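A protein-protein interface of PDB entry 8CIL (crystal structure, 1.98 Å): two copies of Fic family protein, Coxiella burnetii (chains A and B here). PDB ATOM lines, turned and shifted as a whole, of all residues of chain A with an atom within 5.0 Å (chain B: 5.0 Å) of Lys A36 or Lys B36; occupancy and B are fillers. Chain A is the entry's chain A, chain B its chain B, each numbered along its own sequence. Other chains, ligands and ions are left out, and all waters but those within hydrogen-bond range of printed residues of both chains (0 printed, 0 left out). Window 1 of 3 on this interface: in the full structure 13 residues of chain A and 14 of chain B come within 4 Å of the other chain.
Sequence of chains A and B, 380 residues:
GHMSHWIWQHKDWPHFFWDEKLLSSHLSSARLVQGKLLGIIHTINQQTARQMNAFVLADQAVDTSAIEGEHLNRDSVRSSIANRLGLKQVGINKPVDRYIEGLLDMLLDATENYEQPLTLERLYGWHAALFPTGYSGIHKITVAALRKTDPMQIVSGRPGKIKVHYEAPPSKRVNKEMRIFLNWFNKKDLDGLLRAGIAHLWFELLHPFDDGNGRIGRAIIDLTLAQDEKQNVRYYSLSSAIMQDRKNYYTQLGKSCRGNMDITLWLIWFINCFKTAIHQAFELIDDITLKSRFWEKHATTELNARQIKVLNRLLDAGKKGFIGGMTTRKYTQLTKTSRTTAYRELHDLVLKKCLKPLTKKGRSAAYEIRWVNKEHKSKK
Of the 11 printed residues of chain B, 8 touch a printed residue of chain A. Among the printed residues, 17 pairs touch across the chains. Among the printed residues, no Asp or Glu carboxylate lies within 4 Å of a Lys or Arg side-chain nitrogen of the other chain.
Printed residues of chain B within 4 Å of Gly A35: Leu B32 (3.6 Å), Gly B35 (3.3 Å) and Lys B36 (3.2 Å). Lys A36 touches just these residues of chain B: Gly B35, Lys B36, Leu B38 and Gly B39. Leu A38 touches none of the printed residues of chain B. Of the printed residues of chain A, Gly B35 touches Leu A32 (3.6 Å), Gly A35 (3.3 Å) and Lys A36 (3.0 Å). Of the printed residues of chain A, Lys B36 touches Gly A35, Lys A36 and Gly A39. Of the printed residues of chain A, Leu B38 touches Lys A36. Printed residues of chain A within 4 Å of Gly B39: Lys A36 (3.5 Å), Gly A39 (3.8 Å) and Ile A40 (3.7 Å). Printed residues of chain A within 4 Å of Ile B40: Gly A39.
The side-chain amide oxygen (OE1) of Gln B34 sits at hydrogen-bond distance from the guanidinium group (NH1) of Arg B31, at 2.8 Å. OE1 of Gln A34 sits at hydrogen-bond distance from NH1 of Arg A31.
O of Arg A31 touches O of Arg B31, 3.9 Å away. Arg A31 touches Leu B32 (O to CA, 3.6 Å). OE1 of Gln B34 touches CD1 of Leu A32, at 3.6 Å. O of Leu A32 touches CA of Gly B35, 3.6 Å away. Leu B32 touches Gly A35 (O to CA, 3.6 Å). N of Lys B36 touches N of Lys A36, at 3.9 Å. Gly B39 touches Lys A36 (CA to O, 3.5 Å). Gly A39 touches Lys B36. Gly A39 touches Gly B39 (C to C, 3.8 Å). Ile A40 touches Gly B39 (CG1 to O, 3.7 Å).
The backbone carbonyl oxygen of Gly A35 lies close to the backbone carbonyl oxygen of Gly B35 (3.4 Å). N of Lys A36 sits close to O of Gly B35 (3.3 Å). The backbone carbonyl oxygen (O) of Gly A35 lies close to the backbone NH (N) of Lys B36 (3.4 Å).
Leu A32 touches Gln B34, and with the chains exchanged Gln A34 touches Leu B32. Lys B36 touches its own counterpart, Lys A36. Gly B39 touches its own counterpart, Gly A39. Gly A39 touches Ile B40, and with the chains exchanged Ile A40 touches Gly B39. Positions printed for both chains: 31, 32, 33, 34, 35, 36, 37, 38, 39, 40 and 282.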
ATOM      1  N   ARG A  31       7.595 -24.282  -2.052  1.00  0.00           N
ATOM      2  CA  ARG A  31       7.274 -22.958  -1.525  1.00  0.00           C
ATOM      3  C   ARG A  31       6.590 -23.050  -0.162  1.00  0.00           C
ATOM      4  O   ARG A  31       6.804 -22.198   0.707  1.00  0.00           O
ATOM      5  CB  ARG A  31       6.355 -22.196  -2.507  1.00  0.00           C
ATOM      6  CG  ARG A  31       7.073 -21.775  -3.758  1.00  0.00           C
ATOM      7  CD  ARG A  31       8.335 -21.062  -3.528  1.00  0.00           C
ATOM      8  NE  ARG A  31       8.880 -20.466  -4.760  1.00  0.00           N
ATOM      9  CZ  ARG A  31       9.899 -19.595  -4.784  1.00  0.00           C
ATOM     10  NH1 ARG A  31      10.476 -19.232  -3.639  1.00  0.00           N
ATOM     11  NH2 ARG A  31      10.321 -19.039  -5.929  1.00  0.00           N
ATOM     12  N   LEU A  32       5.724 -24.039   0.024  1.00  0.00           N
ATOM     13  CA  LEU A  32       5.039 -24.183   1.307  1.00  0.00           C
ATOM     14  C   LEU A  32       6.044 -24.406   2.451  1.00  0.00           C
ATOM     15  O   LEU A  32       5.933 -23.771   3.506  1.00  0.00           O
ATOM     16  CB  LEU A  32       4.068 -25.350   1.247  1.00  0.00           C
ATOM     17  CG  LEU A  32       3.246 -25.665   2.504  1.00  0.00           C
ATOM     18  CD1 LEU A  32       2.283 -24.474   2.894  1.00  0.00           C
ATOM     19  CD2 LEU A  32       2.377 -26.979   2.339  1.00  0.00           C
ATOM     20  N   VAL A  33       7.012 -25.332   2.282  1.00  0.00           N
ATOM     21  CA  VAL A  33       7.927 -25.570   3.425  1.00  0.00           C
ATOM     22  C   VAL A  33       8.914 -24.417   3.546  1.00  0.00           C
ATOM     23  O   VAL A  33       9.303 -24.036   4.658  1.00  0.00           O
ATOM     24  CB  VAL A  33       8.694 -26.929   3.372  1.00  0.00           C
ATOM     25  CG1 VAL A  33       7.758 -28.062   3.524  1.00  0.00           C
ATOM     26  CG2 VAL A  33       9.435 -27.066   2.083  1.00  0.00           C
ATOM     27  N   GLN A  34       9.325 -23.830   2.424  1.00  0.00           N
ATOM     28  CA  GLN A  34      10.158 -22.636   2.491  1.00  0.00           C
ATOM     29  C   GLN A  34       9.456 -21.528   3.267  1.00  0.00           C
ATOM     30  O   GLN A  34      10.054 -20.890   4.123  1.00  0.00           O
ATOM     31  CB  GLN A  34      10.492 -22.121   1.074  1.00  0.00           C
ATOM     32  CG  GLN A  34      11.337 -20.847   1.028  1.00  0.00           C
ATOM     33  CD  GLN A  34      11.416 -20.229  -0.351  1.00  0.00           C
ATOM     34  OE1 GLN A  34      10.518 -20.404  -1.139  1.00  0.00           O
ATOM     35  NE2 GLN A  34      12.522 -19.553  -0.680  1.00  0.00           N
ATOM     36  N   GLY A  35       8.174 -21.263   2.969  1.00  0.00           N
ATOM     37  CA  GLY A  35       7.485 -20.233   3.726  1.00  0.00           C
ATOM     38  C   GLY A  35       7.394 -20.573   5.198  1.00  0.00           C
ATOM     39  O   GLY A  35       7.582 -19.698   6.061  1.00  0.00           O
ATOM     40  N   LYS A  36       7.137 -21.845   5.512  1.00  0.00           N
ATOM     41  CA  LYS A  36       7.044 -22.218   6.923  1.00  0.00           C
ATOM     42  C   LYS A  36       8.343 -21.857   7.655  1.00  0.00           C
ATOM     43  O   LYS A  36       8.316 -21.276   8.745  1.00  0.00           O
ATOM     44  CB  LYS A  36       6.745 -23.712   7.084  1.00  0.00           C
ATOM     45  CG  LYS A  36       5.328 -24.141   6.832  1.00  0.00           C
ATOM     46  CD  LYS A  36       5.111 -25.643   6.889  1.00  0.00           C
ATOM     47  CE  LYS A  36       3.588 -25.966   6.751  1.00  0.00           C
ATOM     48  NZ  LYS A  36       3.207 -27.395   6.505  1.00  0.00           N
ATOM     49  N   LEU A  37       9.485 -22.226   7.073  1.00  0.00           N
ATOM     50  CA  LEU A  37      10.770 -21.871   7.704  1.00  0.00           C
ATOM     51  C   LEU A  37      10.939 -20.361   7.823  1.00  0.00           C
ATOM     52  O   LEU A  37      11.373 -19.838   8.871  1.00  0.00           O
ATOM     53  CB  LEU A  37      11.931 -22.472   6.890  1.00  0.00           C
ATOM     54  CG  LEU A  37      13.351 -22.201   7.575  1.00  0.00           C
ATOM     55  CD1 LEU A  37      13.404 -22.972   8.941  1.00  0.00           C
ATOM     56  CD2 LEU A  37      14.441 -22.699   6.661  1.00  0.00           C
ATOM     57  N   LEU A  38      10.640 -19.630   6.746  1.00  0.00           N
ATOM     58  CA  LEU A  38      10.788 -18.180   6.781  1.00  0.00           C
ATOM     59  C   LEU A  38       9.873 -17.556   7.839  1.00  0.00           C
ATOM     60  O   LEU A  38      10.208 -16.511   8.425  1.00  0.00           O
ATOM     61  CB  LEU A  38      10.489 -17.589   5.392  1.00  0.00           C
ATOM     62  CG  LEU A  38      11.586 -17.882   4.316  1.00  0.00           C
ATOM     63  CD1 LEU A  38      11.135 -17.438   2.936  1.00  0.00           C
ATOM     64  CD2 LEU A  38      12.881 -17.115   4.640  1.00  0.00           C
ATOM     65  N   GLY A  39       8.677 -18.131   8.049  1.00  0.00           N
ATOM     66  CA  GLY A  39       7.765 -17.567   9.053  1.00  0.00           C
ATOM     67  C   GLY A  39       8.299 -17.837  10.460  1.00  0.00           C
ATOM     68  O   GLY A  39       8.183 -16.992  11.363  1.00  0.00           O
ATOM     69  N   ILE A  40       8.838 -19.026  10.677  1.00  0.00           N
ATOM     70  CA  ILE A  40       9.499 -19.301  11.968  1.00  0.00           C
ATOM     71  C   ILE A  40      10.639 -18.296  12.198  1.00  0.00           C
ATOM     72  O   ILE A  40      10.723 -17.626  13.244  1.00  0.00           O
ATOM     73  CB  ILE A  40      10.022 -20.753  12.013  1.00  0.00           C
ATOM     74  CG1 ILE A  40       8.893 -21.812  11.996  1.00  0.00           C
ATOM     75  CG2 ILE A  40      11.000 -20.968  13.290  1.00  0.00           C
ATOM     76  CD1 ILE A  40       9.541 -23.253  11.733  1.00  0.00           C
ATOM     77  N   PHE A 282      14.346 -27.272   9.927  1.00  0.00           N
ATOM     78  CA  PHE A 282      13.267 -27.401  10.922  1.00  0.00           C
ATOM     79  C   PHE A 282      13.782 -28.102  12.175  1.00  0.00           C
ATOM     80  O   PHE A 282      13.511 -27.672  13.308  1.00  0.00           O
ATOM     81  CB  PHE A 282      12.067 -28.223  10.410  1.00  0.00           C
ATOM     82  CG  PHE A 282      11.208 -27.505   9.409  1.00  0.00           C
ATOM     83  CD1 PHE A 282      10.965 -26.138   9.516  1.00  0.00           C
ATOM     84  CD2 PHE A 282      10.692 -28.190   8.341  1.00  0.00           C
ATOM     85  CE1 PHE A 282      10.153 -25.481   8.556  1.00  0.00           C
ATOM     86  CE2 PHE A 282       9.862 -27.538   7.397  1.00  0.00           C
ATOM     87  CZ  PHE A 282       9.633 -26.195   7.496  1.00  0.00           C
ATOM     88  N   ARG B  31       1.179 -20.715  -1.858  1.00  0.00           N
ATOM     89  CA  ARG B  31       1.790 -21.625  -0.891  1.00  0.00           C
ATOM     90  C   ARG B  31       2.890 -20.940  -0.093  1.00  0.00           C
ATOM     91  O   ARG B  31       3.071 -21.234   1.077  1.00  0.00           O
ATOM     92  CB  ARG B  31       2.402 -22.853  -1.589  1.00  0.00           C
ATOM     93  CG  ARG B  31       1.336 -23.834  -2.139  1.00  0.00           C
ATOM     94  CD  ARG B  31       0.270 -24.171  -1.158  1.00  0.00           C
ATOM     95  NE  ARG B  31      -0.531 -25.304  -1.636  1.00  0.00           N
ATOM     96  CZ  ARG B  31      -1.368 -26.002  -0.862  1.00  0.00           C
ATOM     97  NH1 ARG B  31      -1.503 -25.626   0.426  1.00  0.00           N
ATOM     98  NH2 ARG B  31      -2.065 -27.066  -1.371  1.00  0.00           N
ATOM     99  N   LEU B  32       3.667 -20.071  -0.722  1.00  0.00           N
ATOM    100  CA  LEU B  32       4.721 -19.389  -0.002  1.00  0.00           C
ATOM    101  C   LEU B  32       4.148 -18.539   1.144  1.00  0.00           C
ATOM    102  O   LEU B  32       4.616 -18.638   2.274  1.00  0.00           O
ATOM    103  CB  LEU B  32       5.549 -18.522  -0.962  1.00  0.00           C
ATOM    104  CG  LEU B  32       6.645 -17.681  -0.320  1.00  0.00           C
ATOM    105  CD1 LEU B  32       7.746 -18.664   0.308  1.00  0.00           C
ATOM    106  CD2 LEU B  32       7.438 -16.822  -1.350  1.00  0.00           C
ATOM    107  N   VAL B  33       3.117 -17.721   0.874  1.00  0.00           N
ATOM    108  CA  VAL B  33       2.604 -16.892   1.985  1.00  0.00           C
ATOM    109  C   VAL B  33       1.836 -17.713   3.003  1.00  0.00           C
ATOM    110  O   VAL B  33       1.871 -17.406   4.209  1.00  0.00           O
ATOM    111  CB  VAL B  33       1.728 -15.705   1.514  1.00  0.00           C
ATOM    112  CG1 VAL B  33       2.618 -14.695   0.826  1.00  0.00           C
ATOM    113  CG2 VAL B  33       0.522 -16.132   0.617  1.00  0.00           C
ATOM    114  N   GLN B  34       1.125 -18.747   2.550  1.00  0.00           N
ATOM    115  CA  GLN B  34       0.436 -19.635   3.470  1.00  0.00           C
ATOM    116  C   GLN B  34       1.423 -20.277   4.419  1.00  0.00           C
ATOM    117  O   GLN B  34       1.166 -20.380   5.616  1.00  0.00           O
ATOM    118  CB  GLN B  34      -0.329 -20.731   2.705  1.00  0.00           C
ATOM    119  CG  GLN B  34      -1.019 -21.818   3.635  1.00  0.00           C
ATOM    120  CD  GLN B  34      -1.518 -23.027   2.841  1.00  0.00           C
ATOM    121  OE1 GLN B  34      -0.970 -23.312   1.815  1.00  0.00           O
ATOM    122  NE2 GLN B  34      -2.590 -23.708   3.299  1.00  0.00           N
ATOM    123  N   GLY B  35       2.543 -20.798   3.874  1.00  0.00           N
ATOM    124  CA  GLY B  35       3.611 -21.349   4.727  1.00  0.00           C
ATOM    125  C   GLY B  35       4.143 -20.322   5.719  1.00  0.00           C
ATOM    126  O   GLY B  35       4.436 -20.652   6.885  1.00  0.00           O
ATOM    127  N   LYS B  36       4.327 -19.086   5.270  1.00  0.00           N
ATOM    128  CA  LYS B  36       4.837 -18.078   6.201  1.00  0.00           C
ATOM    129  C   LYS B  36       3.890 -17.919   7.398  1.00  0.00           C
ATOM    130  O   LYS B  36       4.309 -18.004   8.555  1.00  0.00           O
ATOM    131  CB  LYS B  36       5.034 -16.737   5.512  1.00  0.00           C
ATOM    132  CG  LYS B  36       6.242 -16.673   4.620  1.00  0.00           C
ATOM    133  CD  LYS B  36       6.425 -15.307   3.939  1.00  0.00           C
ATOM    134  CE  LYS B  36       7.744 -15.300   3.156  1.00  0.00           C
ATOM    135  NZ  LYS B  36       7.917 -14.161   2.263  1.00  0.00           N
ATOM    136  N   LEU B  37       2.602 -17.727   7.127  1.00  0.00           N
ATOM    137  CA  LEU B  37       1.621 -17.619   8.201  1.00  0.00           C
ATOM    138  C   LEU B  37       1.641 -18.850   9.087  1.00  0.00           C
ATOM    139  O   LEU B  37       1.634 -18.738  10.306  1.00  0.00           O
ATOM    140  CB  LEU B  37       0.199 -17.402   7.604  1.00  0.00           C
ATOM    141  CG  LEU B  37      -0.875 -17.213   8.691  1.00  0.00           C
ATOM    142  CD1 LEU B  37      -0.546 -15.909   9.534  1.00  0.00           C
ATOM    143  CD2 LEU B  37      -2.292 -17.057   7.975  1.00  0.00           C
ATOM    144  N   LEU B  38       1.676 -20.047   8.505  1.00  0.00           N
ATOM    145  CA  LEU B  38       1.686 -21.239   9.332  1.00  0.00           C
ATOM    146  C   LEU B  38       2.951 -21.291  10.200  1.00  0.00           C
ATOM    147  O   LEU B  38       2.914 -21.771  11.333  1.00  0.00           O
ATOM    148  CB  LEU B  38       1.619 -22.505   8.450  1.00  0.00           C
ATOM    149  CG  LEU B  38       0.260 -22.761   7.732  1.00  0.00           C
ATOM    150  CD1 LEU B  38       0.413 -23.977   6.771  1.00  0.00           C
ATOM    151  CD2 LEU B  38      -0.800 -23.032   8.791  1.00  0.00           C
ATOM    152  N   GLY B  39       4.072 -20.800   9.679  1.00  0.00           N
ATOM    153  CA  GLY B  39       5.308 -20.807  10.449  1.00  0.00           C
ATOM    154  C   GLY B  39       5.231 -19.829  11.620  1.00  0.00           C
ATOM    155  O   GLY B  39       5.742 -20.096  12.708  1.00  0.00           O
ATOM    156  N   ILE B  40       4.624 -18.680  11.391  1.00  0.00           N
ATOM    157  CA  ILE B  40       4.370 -17.714  12.474  1.00  0.00           C
ATOM    158  C   ILE B  40       3.481 -18.323  13.568  1.00  0.00           C
ATOM    159  O   ILE B  40       3.804 -18.289  14.758  1.00  0.00           O
ATOM    160  CB  ILE B  40       3.765 -16.443  11.880  1.00  0.00           C
ATOM    161  CG1 ILE B  40       4.793 -15.784  10.949  1.00  0.00           C
ATOM    162  CG2 ILE B  40       3.282 -15.508  12.994  1.00  0.00           C
ATOM    163  CD1 ILE B  40       4.026 -14.694  10.046  1.00  0.00           C
ATOM    164  N   PHE B 282      -1.505 -11.638   8.371  1.00  0.00           N
ATOM    165  CA  PHE B 282      -0.167 -11.133   8.731  1.00  0.00           C
ATOM    166  C   PHE B 282      -0.306  -9.828   9.515  1.00  0.00           C
ATOM    167  O   PHE B 282       0.445  -9.549  10.457  1.00  0.00           O
ATOM    168  CB  PHE B 282       0.689 -10.787   7.489  1.00  0.00           C
ATOM    169  CG  PHE B 282       1.209 -11.971   6.684  1.00  0.00           C
ATOM    170  CD1 PHE B 282       1.604 -13.151   7.308  1.00  0.00           C
ATOM    171  CD2 PHE B 282       1.334 -11.859   5.301  1.00  0.00           C
ATOM    172  CE1 PHE B 282       2.127 -14.239   6.578  1.00  0.00           C
ATOM    173  CE2 PHE B 282       1.873 -12.945   4.552  1.00  0.00           C
ATOM    174  CZ  PHE B 282       2.251 -14.120   5.194  1.00  0.00           C
